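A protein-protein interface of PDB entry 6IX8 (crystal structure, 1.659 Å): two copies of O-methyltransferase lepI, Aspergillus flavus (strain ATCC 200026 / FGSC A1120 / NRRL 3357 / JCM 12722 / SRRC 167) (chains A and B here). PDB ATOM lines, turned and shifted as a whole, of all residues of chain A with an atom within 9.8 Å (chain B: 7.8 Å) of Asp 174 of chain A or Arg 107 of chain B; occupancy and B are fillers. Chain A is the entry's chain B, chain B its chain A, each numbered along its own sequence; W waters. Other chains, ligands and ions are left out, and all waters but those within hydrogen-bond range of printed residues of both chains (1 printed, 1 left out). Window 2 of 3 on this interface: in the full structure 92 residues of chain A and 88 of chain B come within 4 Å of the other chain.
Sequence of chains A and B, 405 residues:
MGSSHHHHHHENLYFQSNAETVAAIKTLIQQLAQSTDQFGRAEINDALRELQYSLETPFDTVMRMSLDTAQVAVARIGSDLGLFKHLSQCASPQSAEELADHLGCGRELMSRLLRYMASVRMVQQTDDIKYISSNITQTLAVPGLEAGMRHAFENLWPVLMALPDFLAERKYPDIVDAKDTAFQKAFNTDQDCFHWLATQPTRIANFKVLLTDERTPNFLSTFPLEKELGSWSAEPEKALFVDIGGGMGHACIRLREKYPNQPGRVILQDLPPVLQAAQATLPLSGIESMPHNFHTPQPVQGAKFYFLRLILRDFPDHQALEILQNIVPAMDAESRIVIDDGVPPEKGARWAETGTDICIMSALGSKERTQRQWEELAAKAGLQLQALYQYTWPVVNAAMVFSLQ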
ATOM      1  N   LEU A 163      -4.703 -36.178  -4.984  1.00  0.00           N
ATOM      2  CA  LEU A 163      -4.069 -35.243  -4.055  1.00  0.00           C
ATOM      3  C   LEU A 163      -4.867 -33.950  -3.869  1.00  0.00           C
ATOM      4  O   LEU A 163      -4.996 -33.525  -2.716  1.00  0.00           O
ATOM      5  CB  LEU A 163      -2.626 -34.930  -4.511  1.00  0.00           C
ATOM      6  CG  LEU A 163      -1.836 -33.977  -3.591  1.00  0.00           C
ATOM      7  CD1 LEU A 163      -1.480 -34.646  -2.265  1.00  0.00           C
ATOM      8  CD2 LEU A 163      -0.548 -33.600  -4.393  1.00  0.00           C
ATOM      9  N   PHE A 166      -7.829 -34.589  -1.635  1.00  0.00           N
ATOM     10  CA  PHE A 166      -7.333 -35.043  -0.336  1.00  0.00           C
ATOM     11  C   PHE A 166      -6.889 -33.859   0.519  1.00  0.00           C
ATOM     12  O   PHE A 166      -7.298 -33.727   1.697  1.00  0.00           O
ATOM     13  CB  PHE A 166      -6.196 -36.034  -0.506  1.00  0.00           C
ATOM     14  CG  PHE A 166      -5.524 -36.405   0.799  1.00  0.00           C
ATOM     15  CD1 PHE A 166      -6.151 -37.289   1.687  1.00  0.00           C
ATOM     16  CD2 PHE A 166      -4.287 -35.862   1.158  1.00  0.00           C
ATOM     17  CE1 PHE A 166      -5.540 -37.599   2.894  1.00  0.00           C
ATOM     18  CE2 PHE A 166      -3.693 -36.190   2.374  1.00  0.00           C
ATOM     19  CZ  PHE A 166      -4.325 -37.059   3.233  1.00  0.00           C
ATOM     20  N   LEU A 167      -6.091 -32.945  -0.073  1.00  0.00           N
ATOM     21  CA  LEU A 167      -5.625 -31.809   0.706  1.00  0.00           C
ATOM     22  C   LEU A 167      -6.766 -30.885   1.064  1.00  0.00           C
ATOM     23  O   LEU A 167      -6.731 -30.269   2.135  1.00  0.00           O
ATOM     24  CB  LEU A 167      -4.550 -31.005  -0.081  1.00  0.00           C
ATOM     25  CG  LEU A 167      -3.260 -31.791  -0.373  1.00  0.00           C
ATOM     26  CD1 LEU A 167      -2.259 -30.998  -1.304  1.00  0.00           C
ATOM     27  CD2 LEU A 167      -2.537 -32.219   0.914  1.00  0.00           C
ATOM     28  N   ARG A 170      -8.892 -32.124   3.962  1.00  0.00           N
ATOM     29  CA  ARG A 170      -8.126 -32.171   5.195  1.00  0.00           C
ATOM     30  C   ARG A 170      -7.500 -30.830   5.568  1.00  0.00           C
ATOM     31  O   ARG A 170      -6.666 -30.777   6.498  1.00  0.00           O
ATOM     32  CB  ARG A 170      -7.079 -33.263   5.083  1.00  0.00           C
ATOM     33  CG  ARG A 170      -7.734 -34.670   5.030  1.00  0.00           C
ATOM     34  CD  ARG A 170      -8.063 -35.197   6.456  1.00  0.00           C
ATOM     35  NE  ARG A 170      -6.836 -35.108   7.218  1.00  0.00           N
ATOM     36  CZ  ARG A 170      -5.934 -36.070   7.260  1.00  0.00           C
ATOM     37  NH1 ARG A 170      -6.172 -37.241   6.678  1.00  0.00           N
ATOM     38  NH2 ARG A 170      -4.818 -35.852   7.931  1.00  0.00           N
ATOM     39  N   LYS A 171      -7.897 -29.763   4.872  1.00  0.00           N
ATOM     40  CA  LYS A 171      -7.490 -28.383   5.150  1.00  0.00           C
ATOM     41  C   LYS A 171      -5.978 -28.260   5.117  1.00  0.00           C
ATOM     42  O   LYS A 171      -5.360 -27.636   5.993  1.00  0.00           O
ATOM     43  CB  LYS A 171      -8.068 -27.881   6.491  1.00  0.00           C
ATOM     44  CG  LYS A 171      -9.602 -27.897   6.500  1.00  0.00           C
ATOM     45  CD  LYS A 171     -10.162 -27.391   7.839  1.00  0.00           C
ATOM     46  CE  LYS A 171     -11.653 -27.037   7.742  1.00  0.00           C
ATOM     47  NZ  LYS A 171     -12.557 -28.219   7.917  1.00  0.00           N
ATOM     48  N   TYR A 172      -5.352 -28.895   4.063  1.00  0.00           N
ATOM     49  CA  TYR A 172      -3.945 -28.671   3.725  1.00  0.00           C
ATOM     50  C   TYR A 172      -3.005 -28.991   4.853  1.00  0.00           C
ATOM     51  O   TYR A 172      -2.198 -28.150   5.276  1.00  0.00           O
ATOM     52  CB  TYR A 172      -3.747 -27.232   3.208  1.00  0.00           C
ATOM     53  CG  TYR A 172      -4.650 -27.051   2.025  1.00  0.00           C
ATOM     54  CD1 TYR A 172      -4.253 -27.471   0.721  1.00  0.00           C
ATOM     55  CD2 TYR A 172      -5.953 -26.573   2.189  1.00  0.00           C
ATOM     56  CE1 TYR A 172      -5.142 -27.384  -0.325  1.00  0.00           C
ATOM     57  CE2 TYR A 172      -6.822 -26.461   1.139  1.00  0.00           C
ATOM     58  CZ  TYR A 172      -6.413 -26.864  -0.148  1.00  0.00           C
ATOM     59  OH  TYR A 172      -7.329 -26.755  -1.216  1.00  0.00           O
ATOM     60  N   PRO A 173      -3.027 -30.246   5.321  1.00  0.00           N
ATOM     61  CA  PRO A 173      -2.065 -30.672   6.327  1.00  0.00           C
ATOM     62  C   PRO A 173      -0.681 -30.868   5.755  1.00  0.00           C
ATOM     63  O   PRO A 173      -0.473 -31.173   4.569  1.00  0.00           O
ATOM     64  CB  PRO A 173      -2.621 -32.023   6.771  1.00  0.00           C
ATOM     65  CG  PRO A 173      -3.186 -32.617   5.480  1.00  0.00           C
ATOM     66  CD  PRO A 173      -3.790 -31.391   4.763  1.00  0.00           C
ATOM     67  N   ASP A 174       0.274 -30.788   6.646  1.00  0.00           N
ATOM     68  CA  ASP A 174       1.599 -31.288   6.343  1.00  0.00           C
ATOM     69  C   ASP A 174       1.551 -32.813   6.327  1.00  0.00           C
ATOM     70  O   ASP A 174       1.150 -33.438   7.315  1.00  0.00           O
ATOM     71  CB  ASP A 174       2.628 -30.777   7.358  1.00  0.00           C
ATOM     72  CG  ASP A 174       2.926 -29.278   7.235  1.00  0.00           C
ATOM     73  OD1 ASP A 174       2.699 -28.630   6.178  1.00  0.00           O
ATOM     74  OD2 ASP A 174       3.430 -28.726   8.230  1.00  0.00           O
ATOM     75  N   ILE A 175       1.929 -33.424   5.195  1.00  0.00           N
ATOM     76  CA  ILE A 175       1.910 -34.883   5.087  1.00  0.00           C
ATOM     77  C   ILE A 175       3.180 -35.423   5.680  1.00  0.00           C
ATOM     78  O   ILE A 175       4.285 -35.017   5.278  1.00  0.00           O
ATOM     79  CB  ILE A 175       1.748 -35.338   3.627  1.00  0.00           C
ATOM     80  CG1 ILE A 175       0.319 -34.983   3.164  1.00  0.00           C
ATOM     81  CG2 ILE A 175       1.919 -36.834   3.550  1.00  0.00           C
ATOM     82  CD1 ILE A 175       0.048 -35.121   1.702  1.00  0.00           C
ATOM     83  N   VAL A 176       3.030 -36.343   6.629  1.00  0.00           N
ATOM     84  CA  VAL A 176       4.127 -36.881   7.409  1.00  0.00           C
ATOM     85  C   VAL A 176       4.070 -38.386   7.584  1.00  0.00           C
ATOM     86  O   VAL A 176       4.996 -38.946   8.166  1.00  0.00           O
ATOM     87  CB  VAL A 176       4.144 -36.221   8.806  1.00  0.00           C
ATOM     88  CG1 VAL A 176       4.523 -34.764   8.673  1.00  0.00           C
ATOM     89  CG2 VAL A 176       2.722 -36.353   9.456  1.00  0.00           C
ATOM     90  N   ASP A 177       2.971 -39.049   7.176  1.00  0.00           N
ATOM     91  CA  ASP A 177       2.737 -40.455   7.507  1.00  0.00           C
ATOM     92  C   ASP A 177       2.378 -41.288   6.271  1.00  0.00           C
ATOM     93  O   ASP A 177       1.456 -40.934   5.524  1.00  0.00           O
ATOM     94  CB  ASP A 177       1.626 -40.499   8.618  1.00  0.00           C
ATOM     95  CG  ASP A 177       1.095 -41.931   8.980  1.00  0.00           C
ATOM     96  OD1 ASP A 177       1.629 -42.997   8.564  1.00  0.00           O
ATOM     97  OD2 ASP A 177       0.047 -41.966   9.703  1.00  0.00           O
ATOM     98  N   ALA A 178       3.068 -42.433   6.084  1.00  0.00           N
ATOM     99  CA  ALA A 178       2.788 -43.269   4.911  1.00  0.00           C
ATOM    100  C   ALA A 178       1.387 -43.846   4.921  1.00  0.00           C
ATOM    101  O   ALA A 178       0.855 -44.194   3.860  1.00  0.00           O
ATOM    102  CB  ALA A 178       3.804 -44.414   4.791  1.00  0.00           C
ATOM    103  N   ASP A 180      -1.276 -42.117   5.902  1.00  0.00           N
ATOM    104  CA  ASP A 180      -2.238 -41.019   5.845  1.00  0.00           C
ATOM    105  C   ASP A 180      -1.824 -40.024   4.753  1.00  0.00           C
ATOM    106  O   ASP A 180      -1.403 -38.903   4.993  1.00  0.00           O
ATOM    107  CB  ASP A 180      -2.375 -40.304   7.195  1.00  0.00           C
ATOM    108  CG  ASP A 180      -3.471 -39.211   7.159  1.00  0.00           C
ATOM    109  OD1 ASP A 180      -4.347 -39.249   6.249  1.00  0.00           O
ATOM    110  OD2 ASP A 180      -3.445 -38.315   8.032  1.00  0.00           O
ATOM    111  N   THR A 181      -1.975 -40.431   3.491  1.00  0.00           N
ATOM    112  CA  THR A 181      -1.636 -39.512   2.414  1.00  0.00           C
ATOM    113  C   THR A 181      -2.585 -39.790   1.241  1.00  0.00           C
ATOM    114  O   THR A 181      -3.635 -40.442   1.405  1.00  0.00           O
ATOM    115  CB  THR A 181      -0.138 -39.626   2.055  1.00  0.00           C
ATOM    116  OG1 THR A 181       0.166 -38.662   1.043  1.00  0.00           O
ATOM    117  CG2 THR A 181       0.291 -41.048   1.641  1.00  0.00           C
ATOM    118  N   ALA A 182      -2.253 -39.242   0.059  1.00  0.00           N
ATOM    119  CA  ALA A 182      -3.238 -39.334  -1.011  1.00  0.00           C
ATOM    120  C   ALA A 182      -3.449 -40.783  -1.458  1.00  0.00           C
ATOM    121  O   ALA A 182      -4.504 -41.134  -1.997  1.00  0.00           O
ATOM    122  CB  ALA A 182      -2.817 -38.419  -2.187  1.00  0.00           C
ATOM    123  N   MET A 361       5.680 -37.725  -1.758  1.00  0.00           N
ATOM    124  CA  MET A 361       4.777 -37.252  -0.707  1.00  0.00           C
ATOM    125  C   MET A 361       3.396 -37.878  -0.864  1.00  0.00           C
ATOM    126  O   MET A 361       2.821 -38.422   0.102  1.00  0.00           O
ATOM    127  CB  MET A 361       4.702 -35.706  -0.732  1.00  0.00           C
ATOM    128  CG  MET A 361       3.715 -35.136   0.386  1.00  0.00           C
ATOM    129  SD  MET A 361       3.560 -33.321   0.084  1.00  0.00           S
ATOM    130  CE  MET A 361       2.347 -33.449  -1.273  1.00  0.00           C
ATOM    131  N   GLY A 365       4.147 -40.764   1.567  1.00  0.00           N
ATOM    132  CA  GLY A 365       4.330 -39.871   2.682  1.00  0.00           C
ATOM    133  C   GLY A 365       5.755 -39.406   2.952  1.00  0.00           C
ATOM    134  O   GLY A 365       5.985 -38.794   3.998  1.00  0.00           O
ATOM    135  N   SER A 366       6.692 -39.583   2.006  1.00  0.00           N
ATOM    136  CA  SER A 366       8.103 -39.314   2.244  1.00  0.00           C
ATOM    137  C   SER A 366       8.475 -37.997   1.558  1.00  0.00           C
ATOM    138  O   SER A 366       7.603 -37.156   1.306  1.00  0.00           O
ATOM    139  CB  SER A 366       8.976 -40.514   1.776  1.00  0.00           C
ATOM    140  OG  SER A 366       8.825 -40.774   0.381  1.00  0.00           O
ATOM    141  N   LYS A 367       9.756 -37.777   1.302  1.00  0.00           N
ATOM    142  CA  LYS A 367      10.181 -36.479   0.804  1.00  0.00           C
ATOM    143  C   LYS A 367      11.610 -36.583   0.272  1.00  0.00           C
ATOM    144  O   LYS A 367      12.366 -37.468   0.691  1.00  0.00           O
ATOM    145  CB  LYS A 367      10.090 -35.395   1.908  1.00  0.00           C
ATOM    146  CG  LYS A 367      11.220 -35.547   2.959  1.00  0.00           C
ATOM    147  CD  LYS A 367      11.076 -34.630   4.202  1.00  0.00           C
ATOM    148  CE  LYS A 367      11.128 -33.179   3.805  1.00  0.00           C
ATOM    149  NZ  LYS A 367      12.452 -32.693   3.304  1.00  0.00           N
ATOM    150  N   SER B  95       7.685 -14.765   1.272  1.00  0.00           N
ATOM    151  CA  SER B  95       8.247 -16.046   1.696  1.00  0.00           C
ATOM    152  C   SER B  95       7.183 -17.142   1.705  1.00  0.00           C
ATOM    153  O   SER B  95       5.967 -16.885   1.716  1.00  0.00           O
ATOM    154  CB  SER B  95       8.832 -15.953   3.103  1.00  0.00           C
ATOM    155  OG  SER B  95       7.769 -15.768   4.026  1.00  0.00           O
ATOM    156  N   ALA B  96       7.658 -18.391   1.766  1.00  0.00           N
ATOM    157  CA  ALA B  96       6.718 -19.510   1.872  1.00  0.00           C
ATOM    158  C   ALA B  96       5.895 -19.433   3.151  1.00  0.00           C
ATOM    159  O   ALA B  96       4.694 -19.693   3.136  1.00  0.00           O
ATOM    160  CB  ALA B  96       7.470 -20.851   1.779  1.00  0.00           C
ATOM    161  N   GLU B  97       6.509 -18.978   4.249  1.00  0.00           N
ATOM    162  CA  GLU B  97       5.766 -18.850   5.501  1.00  0.00           C
ATOM    163  C   GLU B  97       4.648 -17.813   5.373  1.00  0.00           C
ATOM    164  O   GLU B  97       3.503 -18.046   5.800  1.00  0.00           O
ATOM    165  CB  GLU B  97       6.744 -18.479   6.629  1.00  0.00           C
ATOM    166  CG  GLU B  97       7.890 -19.492   6.869  1.00  0.00           C
ATOM    167  CD  GLU B  97       8.911 -19.665   5.694  1.00  0.00           C
ATOM    168  OE1 GLU B  97       9.109 -18.756   4.847  1.00  0.00           O
ATOM    169  OE2 GLU B  97       9.533 -20.755   5.630  1.00  0.00           O
ATOM    170  N   GLU B  98       4.962 -16.656   4.769  1.00  0.00           N
ATOM    171  CA  GLU B  98       3.957 -15.622   4.571  1.00  0.00           C
ATOM    172  C   GLU B  98       2.812 -16.154   3.750  1.00  0.00           C
ATOM    173  O   GLU B  98       1.648 -15.896   4.044  1.00  0.00           O
ATOM    174  CB  GLU B  98       4.565 -14.390   3.877  1.00  0.00           C
ATOM    175  CG  GLU B  98       5.418 -13.542   4.833  1.00  0.00           C
ATOM    176  CD  GLU B  98       6.418 -12.556   4.188  1.00  0.00           C
ATOM    177  OE1 GLU B  98       6.799 -12.675   2.990  1.00  0.00           O
ATOM    178  OE2 GLU B  98       6.848 -11.612   4.925  1.00  0.00           O
ATOM    179  N   LEU B  99       3.122 -16.835   2.633  1.00  0.00           N
ATOM    180  CA  LEU B  99       2.021 -17.300   1.790  1.00  0.00           C
ATOM    181  C   LEU B  99       1.163 -18.350   2.494  1.00  0.00           C
ATOM    182  O   LEU B  99      -0.075 -18.344   2.333  1.00  0.00           O
ATOM    183  CB  LEU B  99       2.607 -17.868   0.478  1.00  0.00           C
ATOM    184  CG  LEU B  99       3.202 -16.759  -0.414  1.00  0.00           C
ATOM    185  CD1 LEU B  99       4.181 -17.342  -1.540  1.00  0.00           C
ATOM    186  CD2 LEU B  99       2.123 -15.952  -1.065  1.00  0.00           C
ATOM    187  N   ALA B 100       1.817 -19.300   3.189  1.00  0.00           N
ATOM    188  CA  ALA B 100       1.101 -20.367   3.907  1.00  0.00           C
ATOM    189  C   ALA B 100       0.137 -19.760   4.923  1.00  0.00           C
ATOM    190  O   ALA B 100      -1.060 -20.076   4.949  1.00  0.00           O
ATOM    191  CB  ALA B 100       2.096 -21.267   4.626  1.00  0.00           C
ATOM    192  N   ASP B 101       0.658 -18.851   5.742  1.00  0.00           N
ATOM    193  CA  ASP B 101      -0.201 -18.218   6.752  1.00  0.00           C
ATOM    194  C   ASP B 101      -1.333 -17.455   6.106  1.00  0.00           C
ATOM    195  O   ASP B 101      -2.467 -17.528   6.562  1.00  0.00           O
ATOM    196  CB  ASP B 101       0.599 -17.285   7.644  1.00  0.00           C
ATOM    197  CG  ASP B 101       1.599 -18.013   8.488  1.00  0.00           C
ATOM    198  OD1 ASP B 101       1.583 -19.271   8.517  1.00  0.00           O
ATOM    199  OD2 ASP B 101       2.436 -17.315   9.114  1.00  0.00           O
ATOM    200  N   GLY B 104      -3.800 -20.198   4.365  1.00  0.00           N
ATOM    201  CA  GLY B 104      -4.350 -21.281   5.152  1.00  0.00           C
ATOM    202  C   GLY B 104      -3.893 -22.641   4.671  1.00  0.00           C
ATOM    203  O   GLY B 104      -4.697 -23.558   4.462  1.00  0.00           O
ATOM    204  N   CYS B 105      -2.582 -22.773   4.541  1.00  0.00           N
ATOM    205  CA  CYS B 105      -1.943 -23.991   4.113  1.00  0.00           C
ATOM    206  C   CYS B 105      -0.876 -24.358   5.128  1.00  0.00           C
ATOM    207  O   CYS B 105      -0.222 -23.475   5.693  1.00  0.00           O
ATOM    208  CB  CYS B 105      -1.345 -23.735   2.706  1.00  0.00           C
ATOM    209  SG  CYS B 105      -0.562 -25.213   1.986  1.00  0.00           S
ATOM    210  N   GLY B 106      -0.670 -25.657   5.349  1.00  0.00           N
ATOM    211  CA  GLY B 106       0.476 -26.067   6.134  1.00  0.00           C
ATOM    212  C   GLY B 106       1.768 -25.452   5.637  1.00  0.00           C
ATOM    213  O   GLY B 106       1.994 -25.395   4.415  1.00  0.00           O
ATOM    214  N   ARG B 107       2.622 -24.994   6.553  1.00  0.00           N
ATOM    215  CA  ARG B 107       3.868 -24.342   6.160  1.00  0.00           C
ATOM    216  C   ARG B 107       4.784 -25.245   5.334  1.00  0.00           C
ATOM    217  O   ARG B 107       5.408 -24.785   4.369  1.00  0.00           O
ATOM    218  CB  ARG B 107       4.627 -23.858   7.399  1.00  0.00           C
ATOM    219  CG  ARG B 107       3.991 -22.623   8.014  1.00  0.00           C
ATOM    220  CD  ARG B 107       5.018 -21.729   8.696  1.00  0.00           C
ATOM    221  NE  ARG B 107       4.350 -20.594   9.334  1.00  0.00           N
ATOM    222  CZ  ARG B 107       4.988 -19.591   9.931  1.00  0.00           C
ATOM    223  NH1 ARG B 107       6.318 -19.569   9.969  1.00  0.00           N
ATOM    224  NH2 ARG B 107       4.290 -18.603  10.483  1.00  0.00           N
ATOM    225  N   GLU B 108       4.966 -26.495   5.749  1.00  0.00           N
ATOM    226  CA  GLU B 108       5.880 -27.362   5.030  1.00  0.00           C
ATOM    227  C   GLU B 108       5.274 -27.750   3.687  1.00  0.00           C
ATOM    228  O   GLU B 108       5.963 -27.709   2.650  1.00  0.00           O
ATOM    229  CB  GLU B 108       6.201 -28.608   5.879  1.00  0.00           C
ATOM    230  CG  GLU B 108       7.304 -29.475   5.297  1.00  0.00           C
ATOM    231  CD  GLU B 108       8.635 -28.760   5.126  1.00  0.00           C
ATOM    232  OE1 GLU B 108       9.496 -29.298   4.380  1.00  0.00           O
ATOM    233  OE2 GLU B 108       8.829 -27.671   5.727  1.00  0.00           O
ATOM    234  N   LEU B 109       3.972 -28.035   3.689  1.00  0.00           N
ATOM    235  CA  LEU B 109       3.289 -28.322   2.427  1.00  0.00           C
ATOM    236  C   LEU B 109       3.417 -27.131   1.479  1.00  0.00           C
ATOM    237  O   LEU B 109       3.709 -27.309   0.292  1.00  0.00           O
ATOM    238  CB  LEU B 109       1.826 -28.640   2.677  1.00  0.00           C
ATOM    239  CG  LEU B 109       0.900 -28.772   1.458  1.00  0.00           C
ATOM    240  CD1 LEU B 109       1.360 -29.959   0.536  1.00  0.00           C
ATOM    241  CD2 LEU B 109      -0.542 -28.988   1.907  1.00  0.00           C
ATOM    242  N   MET B 110       3.154 -25.913   1.984  1.00  0.00           N
ATOM    243  CA  MET B 110       3.284 -24.730   1.134  1.00  0.00           C
ATOM    244  C   MET B 110       4.694 -24.595   0.570  1.00  0.00           C
ATOM    245  O   MET B 110       4.864 -24.316  -0.633  1.00  0.00           O
ATOM    246  CB  MET B 110       2.888 -23.471   1.923  1.00  0.00           C
ATOM    247  CG  MET B 110       3.085 -22.170   1.172  1.00  0.00           C
ATOM    248  SD  MET B 110       2.075 -22.049  -0.290  1.00  0.00           S
ATOM    249  CE  MET B 110       0.583 -21.718   0.340  1.00  0.00           C
ATOM    250  N   SER B 111       5.728 -24.780   1.407  1.00  0.00           N
ATOM    251  CA  SER B 111       7.089 -24.623   0.927  1.00  0.00           C
ATOM    252  C   SER B 111       7.390 -25.627  -0.192  1.00  0.00           C
ATOM    253  O   SER B 111       7.992 -25.265  -1.216  1.00  0.00           O
ATOM    254  CB  SER B 111       8.083 -24.815   2.057  1.00  0.00           C
ATOM    255  OG  SER B 111       9.387 -24.533   1.580  1.00  0.00           O
ATOM    256  N   ARG B 112       6.950 -26.882  -0.015  1.00  0.00           N
ATOM    257  CA  ARG B 112       7.234 -27.925  -0.997  1.00  0.00           C
ATOM    258  C   ARG B 112       6.466 -27.659  -2.302  1.00  0.00           C
ATOM    259  O   ARG B 112       6.996 -27.890  -3.402  1.00  0.00           O
ATOM    260  CB  ARG B 112       6.864 -29.304  -0.424  1.00  0.00           C
ATOM    261  CG  ARG B 112       7.826 -29.637   0.769  1.00  0.00           C
ATOM    262  CD  ARG B 112       7.334 -30.899   1.487  1.00  0.00           C
ATOM    263  NE  ARG B 112       7.536 -32.096   0.652  1.00  0.00           N
ATOM    264  CZ  ARG B 112       7.210 -33.323   1.067  1.00  0.00           C
ATOM    265  NH1 ARG B 112       6.646 -33.510   2.242  1.00  0.00           N
ATOM    266  NH2 ARG B 112       7.453 -34.374   0.327  1.00  0.00           N
ATOM    267  N   LEU B 113       5.222 -27.218  -2.188  1.00  0.00           N
ATOM    268  CA  LEU B 113       4.448 -26.850  -3.392  1.00  0.00           C
ATOM    269  C   LEU B 113       5.092 -25.695  -4.154  1.00  0.00           C
ATOM    270  O   LEU B 113       5.155 -25.726  -5.399  1.00  0.00           O
ATOM    271  CB  LEU B 113       3.018 -26.453  -3.045  1.00  0.00           C
ATOM    272  CG  LEU B 113       2.136 -27.639  -2.614  1.00  0.00           C
ATOM    273  CD1 LEU B 113       0.785 -27.114  -2.016  1.00  0.00           C
ATOM    274  CD2 LEU B 113       1.872 -28.635  -3.790  1.00  0.00           C
ATOM    275  N   LEU B 114       5.553 -24.656  -3.429  1.00  0.00           N
ATOM    276  CA  LEU B 114       6.174 -23.495  -4.093  1.00  0.00           C
ATOM    277  C   LEU B 114       7.472 -23.875  -4.782  1.00  0.00           C
ATOM    278  O   LEU B 114       7.767 -23.364  -5.892  1.00  0.00           O
ATOM    279  CB  LEU B 114       6.449 -22.359  -3.083  1.00  0.00           C
ATOM    280  CG  LEU B 114       5.138 -21.735  -2.628  1.00  0.00           C
ATOM    281  CD1 LEU B 114       5.376 -20.839  -1.371  1.00  0.00           C
ATOM    282  CD2 LEU B 114       4.482 -20.903  -3.730  1.00  0.00           C
HETATM  283  O   HOH W   1      11.594 -30.019   3.100  1.00  0.00           O
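The guanidinium group of Arg 112 of chain B sits at hydrogen-bond distance from the side-chain sulfur of Met 361 of chain A, at 3.8 Å. O of Ser 366 of chain A sits at hydrogen-bond distance from NH2 of Arg 112 of chain B, at 3.0 Å. The backbone NH of Glu 108 of chain B sits at hydrogen-bond distance from the side-chain carboxylate of Asp 174 of chain A (3.1 Å). The side-chain carboxylate of Asp 174 of chain A is in hydrogen-bond range of the backbone NH of Leu 109 of chain B, 2.9 Å away. N of Gly 106 of chain B sits at hydrogen-bond distance from O of Tyr 172 of chain A (2.9 Å).
N of Met 110 of chain B sits at hydrogen-bond distance from SG of Cys 105 of chain B (3.8 Å). The backbone carbonyl oxygen of Met 361 of chain A is in hydrogen-bond range of the side-chain hydroxyl of Thr 181 of chain A (2.8 Å). O of Ala 100 of chain B lies within hydrogen-bond range of N of Cys 105 of chain B, 3.1 Å away. O of Leu 167 of chain A is in hydrogen-bond range of N of Tyr 172 of chain A (2.7 Å). OD2 of Asp 101 of chain B is in salt-bridge range of NH2 of Arg 107 of chain B (2.6 Å).
Leu 109 of chain B touches Leu 167 of chain A (CD2 to CD2, 3.9 Å). CD2 of Tyr 172 of chain A touches O of Gly 104 of chain B (3.98 Å). Tyr 172 of chain A touches Cys 105 of chain B. Tyr 172 of chain A touches Leu 109 of chain B (C to CD2, 3.8 Å). CD2 of Leu 109 of chain B touches O of Pro 173 of chain A (3.4 Å). Asp 174 of chain A touches Gly 106 of chain B (OD1 to C, 3.4 Å). Arg 107 of chain B touches Asp 174 of chain A (N to OD1, 3.7 Å). Lys 367 of chain A touches Arg 112 of chain B (CB to NH2, 3.2 Å).
Of chain B, only Gly 106 (3.4 Å), Arg 107 (3.7 Å), Glu 108 (3.1 Å) and Leu 109 (2.9 Å) come within 4 Å of Asp 174 of chain A. Printed residues of chain B within 4 Å of Met 361 of chain A: Arg 112. Printed residues of chain A within 4 Å of Gly 104 of chain B: Tyr 172. Of chain A, only Asp 174 (3.7 Å) comes within 4 Å of Arg 107 of chain B. Printed residues of chain A within 4 Å of Glu 108 of chain B: Asp 174 (3.1 Å). Printed residues of chain A within 4 Å of Arg 112 of chain B: Met 361 (3.2 Å), Ser 366 (3.0 Å) and Lys 367 (3.2 Å). The nearest residue of chain A that does not touch Arg 107 of chain B is Tyr 172 of chain A (5.9 Å).
Of the 18 printed residues of chain B, 7 touch a printed residue of chain A. Hydrophobic or aromatic side chains of chain B that line the printed part of chain A: Leu 109. Among the printed residues, 13 pairs touch across the chains. Among the printed residues, no Asp or Glu carboxylate lies within 4 Å of a Lys or Arg side-chain nitrogen of the other chain.
No position is printed for both chains. Of the 13 pairs that touch across the chains among the printed residues, none has its exchanged pair printed and touching as well.
Water W1 lies within hydrogen-bond range of the side-chain carboxylate (OE1) of Glu 108 of chain B (2.6 Å) and the side-chain amino group (NZ) of Lys 367 of chain A (2.8 Å).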
